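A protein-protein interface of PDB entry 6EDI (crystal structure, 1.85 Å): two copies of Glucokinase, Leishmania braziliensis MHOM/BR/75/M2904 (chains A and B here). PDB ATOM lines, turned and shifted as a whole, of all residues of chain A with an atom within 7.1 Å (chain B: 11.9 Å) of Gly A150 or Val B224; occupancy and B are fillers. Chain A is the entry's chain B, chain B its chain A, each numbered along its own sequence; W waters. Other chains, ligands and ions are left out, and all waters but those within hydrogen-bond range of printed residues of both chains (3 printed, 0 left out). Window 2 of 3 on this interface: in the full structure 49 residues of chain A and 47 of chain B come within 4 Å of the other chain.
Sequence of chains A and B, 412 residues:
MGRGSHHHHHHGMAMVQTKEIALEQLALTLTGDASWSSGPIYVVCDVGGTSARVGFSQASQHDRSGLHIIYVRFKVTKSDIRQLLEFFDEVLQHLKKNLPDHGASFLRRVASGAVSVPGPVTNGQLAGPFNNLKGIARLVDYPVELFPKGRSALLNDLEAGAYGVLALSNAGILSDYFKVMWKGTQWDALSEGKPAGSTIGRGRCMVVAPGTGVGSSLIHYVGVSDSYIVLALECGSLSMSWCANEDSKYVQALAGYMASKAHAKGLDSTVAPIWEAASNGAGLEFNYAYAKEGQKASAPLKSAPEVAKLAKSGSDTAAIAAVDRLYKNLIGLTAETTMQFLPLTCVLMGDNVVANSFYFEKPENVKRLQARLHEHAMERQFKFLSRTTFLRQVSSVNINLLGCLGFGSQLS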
ATOM      1  N   ALA A 111     -10.312 -34.322 -21.618  1.00  0.00           N
ATOM      2  CA  ALA A 111     -10.472 -33.466 -22.789  1.00  0.00           C
ATOM      3  C   ALA A 111     -10.233 -31.992 -22.473  1.00  0.00           C
ATOM      4  O   ALA A 111      -9.981 -31.188 -23.373  1.00  0.00           O
ATOM      5  CB  ALA A 111     -11.858 -33.657 -23.390  1.00  0.00           C
ATOM      6  N   ASN A 123      -7.511 -13.079 -18.635  1.00  0.00           N
ATOM      7  CA  ASN A 123      -7.211 -13.856 -19.833  1.00  0.00           C
ATOM      8  C   ASN A 123      -7.307 -15.367 -19.655  1.00  0.00           C
ATOM      9  O   ASN A 123      -6.649 -16.125 -20.376  1.00  0.00           O
ATOM     10  CB  ASN A 123      -5.822 -13.466 -20.378  1.00  0.00           C
ATOM     11  CG  ASN A 123      -5.797 -12.056 -20.900  1.00  0.00           C
ATOM     12  OD1 ASN A 123      -6.847 -11.484 -21.153  1.00  0.00           O
ATOM     13  ND2 ASN A 123      -4.604 -11.484 -21.058  1.00  0.00           N
ATOM     14  N   GLY A 124      -8.108 -15.793 -18.675  1.00  0.00           N
ATOM     15  CA  GLY A 124      -8.280 -17.200 -18.361  1.00  0.00           C
ATOM     16  C   GLY A 124      -7.059 -17.858 -17.740  1.00  0.00           C
ATOM     17  O   GLY A 124      -7.004 -19.079 -17.590  1.00  0.00           O
ATOM     18  N   GLN A 125      -6.075 -17.053 -17.355  1.00  0.00           N
ATOM     19  CA  GLN A 125      -4.775 -17.602 -17.013  1.00  0.00           C
ATOM     20  C   GLN A 125      -4.331 -17.240 -15.601  1.00  0.00           C
ATOM     21  O   GLN A 125      -3.505 -17.926 -15.001  1.00  0.00           O
ATOM     22  CB  GLN A 125      -3.743 -17.133 -18.042  1.00  0.00           C
ATOM     23  CG  GLN A 125      -3.865 -17.840 -19.384  1.00  0.00           C
ATOM     24  CD  GLN A 125      -3.192 -17.087 -20.506  1.00  0.00           C
ATOM     25  OE1 GLN A 125      -2.840 -15.922 -20.357  1.00  0.00           O
ATOM     26  NE2 GLN A 125      -3.013 -17.751 -21.640  1.00  0.00           N
ATOM     27  N   LEU A 139      -2.808 -20.523 -13.822  1.00  0.00           N
ATOM     28  CA  LEU A 139      -3.126 -21.698 -14.628  1.00  0.00           C
ATOM     29  C   LEU A 139      -1.848 -22.376 -15.074  1.00  0.00           C
ATOM     30  O   LEU A 139      -1.756 -23.605 -15.070  1.00  0.00           O
ATOM     31  CB  LEU A 139      -3.984 -21.340 -15.843  1.00  0.00           C
ATOM     32  CG  LEU A 139      -4.184 -22.495 -16.834  1.00  0.00           C
ATOM     33  CD1 LEU A 139      -5.200 -23.499 -16.319  1.00  0.00           C
ATOM     34  CD2 LEU A 139      -4.616 -21.953 -18.181  1.00  0.00           C
ATOM     35  N   PHE A 147      -5.107 -30.505 -16.370  1.00  0.00           N
ATOM     36  CA  PHE A 147      -5.357 -29.271 -17.096  1.00  0.00           C
ATOM     37  C   PHE A 147      -4.471 -29.213 -18.332  1.00  0.00           C
ATOM     38  O   PHE A 147      -3.418 -28.571 -18.322  1.00  0.00           O
ATOM     39  CB  PHE A 147      -5.127 -28.074 -16.175  1.00  0.00           C
ATOM     40  CG  PHE A 147      -5.930 -28.139 -14.913  1.00  0.00           C
ATOM     41  CD1 PHE A 147      -7.232 -27.662 -14.887  1.00  0.00           C
ATOM     42  CD2 PHE A 147      -5.397 -28.697 -13.758  1.00  0.00           C
ATOM     43  CE1 PHE A 147      -7.995 -27.732 -13.743  1.00  0.00           C
ATOM     44  CE2 PHE A 147      -6.158 -28.763 -12.589  1.00  0.00           C
ATOM     45  CZ  PHE A 147      -7.458 -28.276 -12.587  1.00  0.00           C
ATOM     46  N   PRO A 148      -4.905 -29.893 -19.406  1.00  0.00           N
ATOM     47  CA  PRO A 148      -4.078 -30.023 -20.610  1.00  0.00           C
ATOM     48  C   PRO A 148      -3.784 -28.668 -21.246  1.00  0.00           C
ATOM     49  O   PRO A 148      -4.635 -27.773 -21.240  1.00  0.00           O
ATOM     50  CB  PRO A 148      -4.942 -30.875 -21.555  1.00  0.00           C
ATOM     51  CG  PRO A 148      -6.033 -31.456 -20.721  1.00  0.00           C
ATOM     52  CD  PRO A 148      -6.228 -30.518 -19.567  1.00  0.00           C
ATOM     53  N   LYS A 149      -2.575 -28.524 -21.785  1.00  0.00           N
ATOM     54  CA  LYS A 149      -2.169 -27.287 -22.430  1.00  0.00           C
ATOM     55  C   LYS A 149      -3.054 -27.011 -23.627  1.00  0.00           C
ATOM     56  O   LYS A 149      -3.318 -27.921 -24.423  1.00  0.00           O
ATOM     57  CB  LYS A 149      -0.713 -27.379 -22.885  1.00  0.00           C
ATOM     58  CG  LYS A 149       0.209 -26.411 -22.171  1.00  0.00           C
ATOM     59  CD  LYS A 149       1.313 -25.961 -23.111  1.00  0.00           C
ATOM     60  CE  LYS A 149       0.723 -25.464 -24.426  1.00  0.00           C
ATOM     61  NZ  LYS A 149       1.673 -25.674 -25.550  1.00  0.00           N
ATOM     62  N   GLY A 150      -3.513 -25.759 -23.735  1.00  0.00           N
ATOM     63  CA  GLY A 150      -4.356 -25.311 -24.832  1.00  0.00           C
ATOM     64  C   GLY A 150      -5.811 -25.690 -24.633  1.00  0.00           C
ATOM     65  O   GLY A 150      -6.665 -25.381 -25.458  1.00  0.00           O
ATOM     66  N   ARG A 151      -6.101 -26.355 -23.521  1.00  0.00           N
ATOM     67  CA  ARG A 151      -7.414 -26.948 -23.312  1.00  0.00           C
ATOM     68  C   ARG A 151      -8.000 -26.587 -21.940  1.00  0.00           C
ATOM     69  O   ARG A 151      -8.960 -27.205 -21.482  1.00  0.00           O
ATOM     70  CB  ARG A 151      -7.292 -28.469 -23.441  1.00  0.00           C
ATOM     71  CG  ARG A 151      -7.347 -29.005 -24.869  1.00  0.00           C
ATOM     72  CD  ARG A 151      -8.809 -29.137 -25.239  1.00  0.00           C
ATOM     73  NE  ARG A 151      -9.098 -29.891 -26.453  1.00  0.00           N
ATOM     74  CZ  ARG A 151      -9.288 -29.327 -27.641  1.00  0.00           C
ATOM     75  NH1 ARG A 151      -9.191 -28.010 -27.768  1.00  0.00           N
ATOM     76  NH2 ARG A 151      -9.558 -30.074 -28.702  1.00  0.00           N
ATOM     77  N   SER A 152      -7.434 -25.572 -21.300  1.00  0.00           N
ATOM     78  CA  SER A 152      -7.769 -25.268 -19.915  1.00  0.00           C
ATOM     79  C   SER A 152      -7.953 -23.789 -19.658  1.00  0.00           C
ATOM     80  O   SER A 152      -7.441 -22.949 -20.395  1.00  0.00           O
ATOM     81  CB  SER A 152      -6.678 -25.780 -18.984  1.00  0.00           C
ATOM     82  OG  SER A 152      -6.546 -27.180 -19.092  1.00  0.00           O
ATOM     83  N   ALA A 153      -8.664 -23.474 -18.585  1.00  0.00           N
ATOM     84  CA  ALA A 153      -8.889 -22.087 -18.235  1.00  0.00           C
ATOM     85  C   ALA A 153      -9.306 -21.934 -16.780  1.00  0.00           C
ATOM     86  O   ALA A 153      -9.969 -22.799 -16.215  1.00  0.00           O
ATOM     87  CB  ALA A 153      -9.951 -21.479 -19.152  1.00  0.00           C
ATOM     88  N   LEU A 154      -8.920 -20.816 -16.188  1.00  0.00           N
ATOM     89  CA  LEU A 154      -9.585 -20.347 -14.984  1.00  0.00           C
ATOM     90  C   LEU A 154     -10.816 -19.587 -15.461  1.00  0.00           C
ATOM     91  O   LEU A 154     -10.738 -18.818 -16.427  1.00  0.00           O
ATOM     92  CB  LEU A 154      -8.656 -19.424 -14.197  1.00  0.00           C
ATOM     93  CG  LEU A 154      -7.358 -20.046 -13.676  1.00  0.00           C
ATOM     94  CD1 LEU A 154      -6.508 -19.007 -12.971  1.00  0.00           C
ATOM     95  CD2 LEU A 154      -7.674 -21.146 -12.720  1.00  0.00           C
ATOM     96  N   LEU A 155     -11.946 -19.813 -14.795  1.00  0.00           N
ATOM     97  CA  LEU A 155     -13.200 -19.158 -15.128  1.00  0.00           C
ATOM     98  C   LEU A 155     -13.672 -18.376 -13.928  1.00  0.00           C
ATOM     99  O   LEU A 155     -13.580 -18.850 -12.787  1.00  0.00           O
ATOM    100  CB  LEU A 155     -14.265 -20.196 -15.517  1.00  0.00           C
ATOM    101  CG  LEU A 155     -13.885 -21.198 -16.619  1.00  0.00           C
ATOM    102  CD1 LEU A 155     -14.968 -22.256 -16.848  1.00  0.00           C
ATOM    103  CD2 LEU A 155     -13.546 -20.487 -17.923  1.00  0.00           C
ATOM    104  N   PHE A 407     -17.528 -25.495 -20.693  1.00  0.00           N
ATOM    105  CA  PHE A 407     -16.288 -24.956 -21.216  1.00  0.00           C
ATOM    106  C   PHE A 407     -15.547 -25.952 -22.117  1.00  0.00           C
ATOM    107  O   PHE A 407     -15.221 -25.618 -23.238  1.00  0.00           O
ATOM    108  CB  PHE A 407     -15.379 -24.468 -20.076  1.00  0.00           C
ATOM    109  CG  PHE A 407     -13.979 -24.153 -20.524  1.00  0.00           C
ATOM    110  CD1 PHE A 407     -13.680 -22.926 -21.123  1.00  0.00           C
ATOM    111  CD2 PHE A 407     -12.970 -25.093 -20.379  1.00  0.00           C
ATOM    112  CE1 PHE A 407     -12.378 -22.647 -21.551  1.00  0.00           C
ATOM    113  CE2 PHE A 407     -11.677 -24.832 -20.800  1.00  0.00           C
ATOM    114  CZ  PHE A 407     -11.378 -23.605 -21.401  1.00  0.00           C
ATOM    115  N   LEU A 411     -14.573 -26.182 -26.895  1.00  0.00           N
ATOM    116  CA  LEU A 411     -13.206 -26.024 -27.384  1.00  0.00           C
ATOM    117  C   LEU A 411     -13.091 -26.377 -28.863  1.00  0.00           C
ATOM    118  O   LEU A 411     -13.740 -27.311 -29.339  1.00  0.00           O
ATOM    119  CB  LEU A 411     -12.260 -26.892 -26.556  1.00  0.00           C
ATOM    120  CG  LEU A 411     -11.990 -26.326 -25.167  1.00  0.00           C
ATOM    121  CD1 LEU A 411     -11.494 -27.392 -24.200  1.00  0.00           C
ATOM    122  CD2 LEU A 411     -10.983 -25.202 -25.289  1.00  0.00           C
ATOM    123  N   SER A 412     -12.271 -25.620 -29.587  1.00  0.00           N
ATOM    124  CA  SER A 412     -12.047 -25.874 -31.007  1.00  0.00           C
ATOM    125  C   SER A 412     -11.087 -27.046 -31.192  1.00  0.00           C
ATOM    126  O   SER A 412     -11.145 -28.027 -30.454  1.00  0.00           O
ATOM    127  CB  SER A 412     -11.512 -24.622 -31.716  1.00  0.00           C
ATOM    128  OG  SER A 412     -10.232 -24.263 -31.223  1.00  0.00           O
ATOM    129  N   ARG B 202      -2.557  -8.041 -25.462  1.00  0.00           N
ATOM    130  CA  ARG B 202      -3.349  -9.231 -25.145  1.00  0.00           C
ATOM    131  C   ARG B 202      -4.360  -8.975 -24.027  1.00  0.00           C
ATOM    132  O   ARG B 202      -4.139  -9.333 -22.859  1.00  0.00           O
ATOM    133  CB  ARG B 202      -2.443 -10.401 -24.760  1.00  0.00           C
ATOM    134  CG  ARG B 202      -1.448 -10.759 -25.840  1.00  0.00           C
ATOM    135  CD  ARG B 202      -1.579 -12.209 -26.253  1.00  0.00           C
ATOM    136  NE  ARG B 202      -0.779 -12.491 -27.439  1.00  0.00           N
ATOM    137  CZ  ARG B 202       0.307 -13.248 -27.444  1.00  0.00           C
ATOM    138  NH1 ARG B 202       0.716 -13.835 -26.324  1.00  0.00           N
ATOM    139  NH2 ARG B 202       0.973 -13.437 -28.575  1.00  0.00           N
ATOM    140  N   GLY B 203      -5.473  -8.356 -24.402  1.00  0.00           N
ATOM    141  CA  GLY B 203      -6.555  -8.070 -23.481  1.00  0.00           C
ATOM    142  C   GLY B 203      -7.722  -7.492 -24.249  1.00  0.00           C
ATOM    143  O   GLY B 203      -7.656  -7.328 -25.477  1.00  0.00           O
ATOM    144  N   HIS B 220     -12.675  -9.031 -27.875  1.00  0.00           N
ATOM    145  CA  HIS B 220     -12.433  -9.865 -26.688  1.00  0.00           C
ATOM    146  C   HIS B 220     -11.224 -10.749 -26.940  1.00  0.00           C
ATOM    147  O   HIS B 220     -11.157 -11.418 -27.970  1.00  0.00           O
ATOM    148  CB  HIS B 220     -13.663 -10.712 -26.382  1.00  0.00           C
ATOM    149  CG  HIS B 220     -13.449 -11.716 -25.283  1.00  0.00           C
ATOM    150  ND1 HIS B 220     -13.241 -11.350 -23.975  1.00  0.00           N
ATOM    151  CD2 HIS B 220     -13.424 -13.069 -25.307  1.00  0.00           C
ATOM    152  CE1 HIS B 220     -13.088 -12.435 -23.231  1.00  0.00           C
ATOM    153  NE2 HIS B 220     -13.202 -13.489 -24.014  1.00  0.00           N
ATOM    154  N   TYR B 221     -10.252 -10.724 -26.027  1.00  0.00           N
ATOM    155  CA  TYR B 221      -9.082 -11.584 -26.154  1.00  0.00           C
ATOM    156  C   TYR B 221      -9.351 -12.908 -25.468  1.00  0.00           C
ATOM    157  O   TYR B 221      -9.877 -12.935 -24.358  1.00  0.00           O
ATOM    158  CB  TYR B 221      -7.821 -10.946 -25.559  1.00  0.00           C
ATOM    159  CG  TYR B 221      -6.662 -11.916 -25.553  1.00  0.00           C
ATOM    160  CD1 TYR B 221      -6.034 -12.286 -26.729  1.00  0.00           C
ATOM    161  CD2 TYR B 221      -6.218 -12.486 -24.368  1.00  0.00           C
ATOM    162  CE1 TYR B 221      -4.991 -13.185 -26.733  1.00  0.00           C
ATOM    163  CE2 TYR B 221      -5.174 -13.391 -24.364  1.00  0.00           C
ATOM    164  CZ  TYR B 221      -4.565 -13.732 -25.547  1.00  0.00           C
ATOM    165  OH  TYR B 221      -3.526 -14.624 -25.551  1.00  0.00           O
ATOM    166  N   VAL B 222      -8.985 -13.992 -26.146  1.00  0.00           N
ATOM    167  CA  VAL B 222      -9.258 -15.356 -25.696  1.00  0.00           C
ATOM    168  C   VAL B 222      -7.950 -16.092 -25.386  1.00  0.00           C
ATOM    169  O   VAL B 222      -7.242 -16.541 -26.296  1.00  0.00           O
ATOM    170  CB  VAL B 222     -10.035 -16.160 -26.770  1.00  0.00           C
ATOM    171  CG1 VAL B 222     -10.282 -17.568 -26.272  1.00  0.00           C
ATOM    172  CG2 VAL B 222     -11.360 -15.479 -27.145  1.00  0.00           C
ATOM    173  N   GLY B 223      -7.627 -16.238 -24.105  1.00  0.00           N
ATOM    174  CA  GLY B 223      -6.341 -16.801 -23.721  1.00  0.00           C
ATOM    175  C   GLY B 223      -6.095 -18.239 -24.161  1.00  0.00           C
ATOM    176  O   GLY B 223      -4.959 -18.606 -24.503  1.00  0.00           O
ATOM    177  N   VAL B 224      -7.158 -19.045 -24.164  1.00  0.00           N
ATOM    178  CA  VAL B 224      -7.063 -20.474 -24.478  1.00  0.00           C
ATOM    179  C   VAL B 224      -6.469 -20.698 -25.854  1.00  0.00           C
ATOM    180  O   VAL B 224      -5.588 -21.537 -26.031  1.00  0.00           O
ATOM    181  CB  VAL B 224      -8.444 -21.159 -24.442  1.00  0.00           C
ATOM    182  CG1 VAL B 224      -8.287 -22.664 -24.565  1.00  0.00           C
ATOM    183  CG2 VAL B 224      -9.182 -20.821 -23.166  1.00  0.00           C
ATOM    184  N   SER B 225      -6.947 -19.915 -26.820  1.00  0.00           N
ATOM    185  CA  SER B 225      -6.571 -20.066 -28.217  1.00  0.00           C
ATOM    186  C   SER B 225      -5.634 -18.967 -28.690  1.00  0.00           C
ATOM    187  O   SER B 225      -5.253 -18.938 -29.865  1.00  0.00           O
ATOM    188  CB  SER B 225      -7.824 -20.074 -29.101  1.00  0.00           C
ATOM    189  OG  SER B 225      -8.557 -18.854 -28.995  1.00  0.00           O
ATOM    190  N   ASP B 226      -5.279 -18.067 -27.777  1.00  0.00           N
ATOM    191  CA  ASP B 226      -4.455 -16.895 -28.088  1.00  0.00           C
ATOM    192  C   ASP B 226      -4.998 -16.178 -29.319  1.00  0.00           C
ATOM    193  O   ASP B 226      -4.280 -15.940 -30.299  1.00  0.00           O
ATOM    194  CB  ASP B 226      -2.986 -17.291 -28.275  1.00  0.00           C
ATOM    195  CG  ASP B 226      -2.081 -16.092 -28.441  1.00  0.00           C
ATOM    196  OD1 ASP B 226      -2.383 -15.039 -27.843  1.00  0.00           O
ATOM    197  OD2 ASP B 226      -1.079 -16.196 -29.179  1.00  0.00           O
ATOM    198  N   SER B 227      -6.289 -15.871 -29.283  1.00  0.00           N
ATOM    199  CA  SER B 227      -6.936 -15.264 -30.438  1.00  0.00           C
ATOM    200  C   SER B 227      -7.941 -14.254 -29.935  1.00  0.00           C
ATOM    201  O   SER B 227      -8.221 -14.186 -28.729  1.00  0.00           O
ATOM    202  CB  SER B 227      -7.648 -16.324 -31.275  1.00  0.00           C
ATOM    203  OG  SER B 227      -8.569 -17.017 -30.465  1.00  0.00           O
ATOM    204  N   TYR B 228      -8.487 -13.469 -30.853  1.00  0.00           N
ATOM    205  CA  TYR B 228      -9.478 -12.469 -30.481  1.00  0.00           C
ATOM    206  C   TYR B 228     -10.799 -12.722 -31.202  1.00  0.00           C
ATOM    207  O   TYR B 228     -10.822 -13.274 -32.306  1.00  0.00           O
ATOM    208  CB  TYR B 228      -8.993 -11.077 -30.901  1.00  0.00           C
ATOM    209  CG  TYR B 228      -7.680 -10.598 -30.315  1.00  0.00           C
ATOM    210  CD1 TYR B 228      -6.453 -11.041 -30.816  1.00  0.00           C
ATOM    211  CD2 TYR B 228      -7.667  -9.647 -29.317  1.00  0.00           C
ATOM    212  CE1 TYR B 228      -5.247 -10.567 -30.286  1.00  0.00           C
ATOM    213  CE2 TYR B 228      -6.475  -9.159 -28.790  1.00  0.00           C
ATOM    214  CZ  TYR B 228      -5.280  -9.616 -29.278  1.00  0.00           C
ATOM    215  OH  TYR B 228      -4.115  -9.120 -28.725  1.00  0.00           O
ATOM    216  N   ILE B 229     -11.905 -12.284 -30.603  1.00  0.00           N
ATOM    217  CA  ILE B 229     -13.176 -12.312 -31.306  1.00  0.00           C
ATOM    218  C   ILE B 229     -13.854 -10.987 -31.027  1.00  0.00           C
ATOM    219  O   ILE B 229     -13.763 -10.459 -29.925  1.00  0.00           O
ATOM    220  CB  ILE B 229     -14.070 -13.514 -30.880  1.00  0.00           C
ATOM    221  CG1 ILE B 229     -15.387 -13.522 -31.664  1.00  0.00           C
ATOM    222  CG2 ILE B 229     -14.306 -13.537 -29.351  1.00  0.00           C
ATOM    223  CD1 ILE B 229     -16.123 -14.861 -31.612  1.00  0.00           C
ATOM    224  N   GLN B 410      -8.335 -14.068 -37.615  1.00  0.00           N
ATOM    225  CA  GLN B 410      -8.641 -14.673 -36.323  1.00  0.00           C
ATOM    226  C   GLN B 410      -9.343 -16.017 -36.456  1.00  0.00           C
ATOM    227  O   GLN B 410      -9.785 -16.582 -35.464  1.00  0.00           O
ATOM    228  CB  GLN B 410      -9.515 -13.732 -35.489  1.00  0.00           C
ATOM    229  CG  GLN B 410      -8.797 -12.470 -35.073  1.00  0.00           C
ATOM    230  CD  GLN B 410      -7.409 -12.765 -34.514  1.00  0.00           C
ATOM    231  OE1 GLN B 410      -7.263 -13.400 -33.460  1.00  0.00           O
ATOM    232  NE2 GLN B 410      -6.381 -12.324 -35.230  1.00  0.00           N
ATOM    233  N   SER B 412     -10.114 -19.879 -36.668  1.00  0.00           N
ATOM    234  CA  SER B 412      -9.493 -21.083 -36.121  1.00  0.00           C
ATOM    235  C   SER B 412      -9.195 -22.079 -37.227  1.00  0.00           C
ATOM    236  O   SER B 412      -8.041 -22.396 -37.483  1.00  0.00           O
ATOM    237  CB  SER B 412     -10.386 -21.734 -35.056  1.00  0.00           C
ATOM    238  OG  SER B 412     -11.582 -22.240 -35.628  1.00  0.00           O
HETATM  239  O   HOH W   1      -6.659 -20.188 -20.962  1.00  0.00           O
HETATM  240  O   HOH W   2      -1.802  -9.587 -21.369  1.00  0.00           O
HETATM  241  O   HOH W   3      -9.336 -14.735 -22.130  1.00  0.00           O
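ND2 of Asn A123 is in hydrogen-bond range of O of Arg B202.
Position printed for both chains: 412.
Printed residues of chain A that touch a printed residue of chain B: Asn A123, Gln A125, Gly A150, Ser A152, Phe A407 and Leu A411. Of the 14 printed residues of chain B, 4 touch a printed residue of chain A. Hydrophobic or aromatic side chains of chain B that line the printed part of chain A: Tyr B221 and Val B224. Along chain B the printed residues that touch a printed residue of chain A span positions 202 to 224. Among the printed residues, 8 pairs touch across the chains.
CD2 of Tyr B221 touches OD1 of Asn A123, at 3.4 Å. Asn A123 touches Gly B223. Gln A125 touches Gly B223. Gly A150 touches Val B224 (O to CG1, 3.3 Å). Ser A152 touches Val B224. Phe A407 touches Val B224 (CZ to CG2, 3.96 Å). CD2 of Leu A411 touches CG1 of Val B224, at 3.8 Å.
O of Gln A125 is in hydrogen-bond range of N of Leu A139 (2.9 Å). O of Pro A148 sits at hydrogen-bond distance from OG of Ser A152 (2.9 Å). The side-chain carboxylate (OD1) of Asp B226 lies within hydrogen-bond range of the side-chain hydroxyl (OH) of Tyr B221, at 2.6 Å. The guanidinium group (NE) of Arg B202 lies within salt-bridge range of the side-chain carboxylate (OD1) of Asp B226.
Water W2 lies within hydrogen-bond range of the backbone carbonyl oxygen of Arg B202 (2.8 Å) and the side-chain amide nitrogen of Asn A123 (3.4 Å). Water W3 lies within hydrogen-bond range of the backbone carbonyl oxygen (O) of Tyr B221 (2.9 Å), the backbone NH (N) of Gly B223 (3.0 Å) and the backbone carbonyl oxygen (O) of Asn A123 (3.5 Å). Water W1 lies within hydrogen-bond range of O of Ser A152 and N of Val B224.
Printed residues of chain B within 4 Å of Gly A150: Val B224 (3.3 Å). Of chain A, only Gly A150, Ser A152, Phe A407 and Leu A411 come within 4 Å of Val B224. No residue of chain B comes within 4 Å of Pro A148. Lys A149 touches none of the printed residues of chain B. Ser A152 touches just one residue of chain B: Val B224 (3.9 Å). Ala A153 touches none of the printed residues of chain B. Of chain A, only Asn A123 and Gln A125 come within 4 Å of Gly B223. Printed residues of chain A within 4 Å of Arg B202: Asn A123. Printed residues of chain B within 4 Å of Asn A123: Arg B202 (2.8 Å), Tyr B221 (3.4 Å) and Gly B223 (3.4 Å). Printed residues of chain B within 4 Å of Phe A407: Val B224 (3.96 Å). Leu A155 touches none of the printed residues of chain B. The nearest residue of chain B that does not touch Gly A150 is Ser B225 (5.6 Å). The nearest residue of chain A that does not touch Val B224 is Ala A153 (4.1 Å). The nearest printed residue of chain A that does not touch Arg B202 is Gln A125 (7.1 Å).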
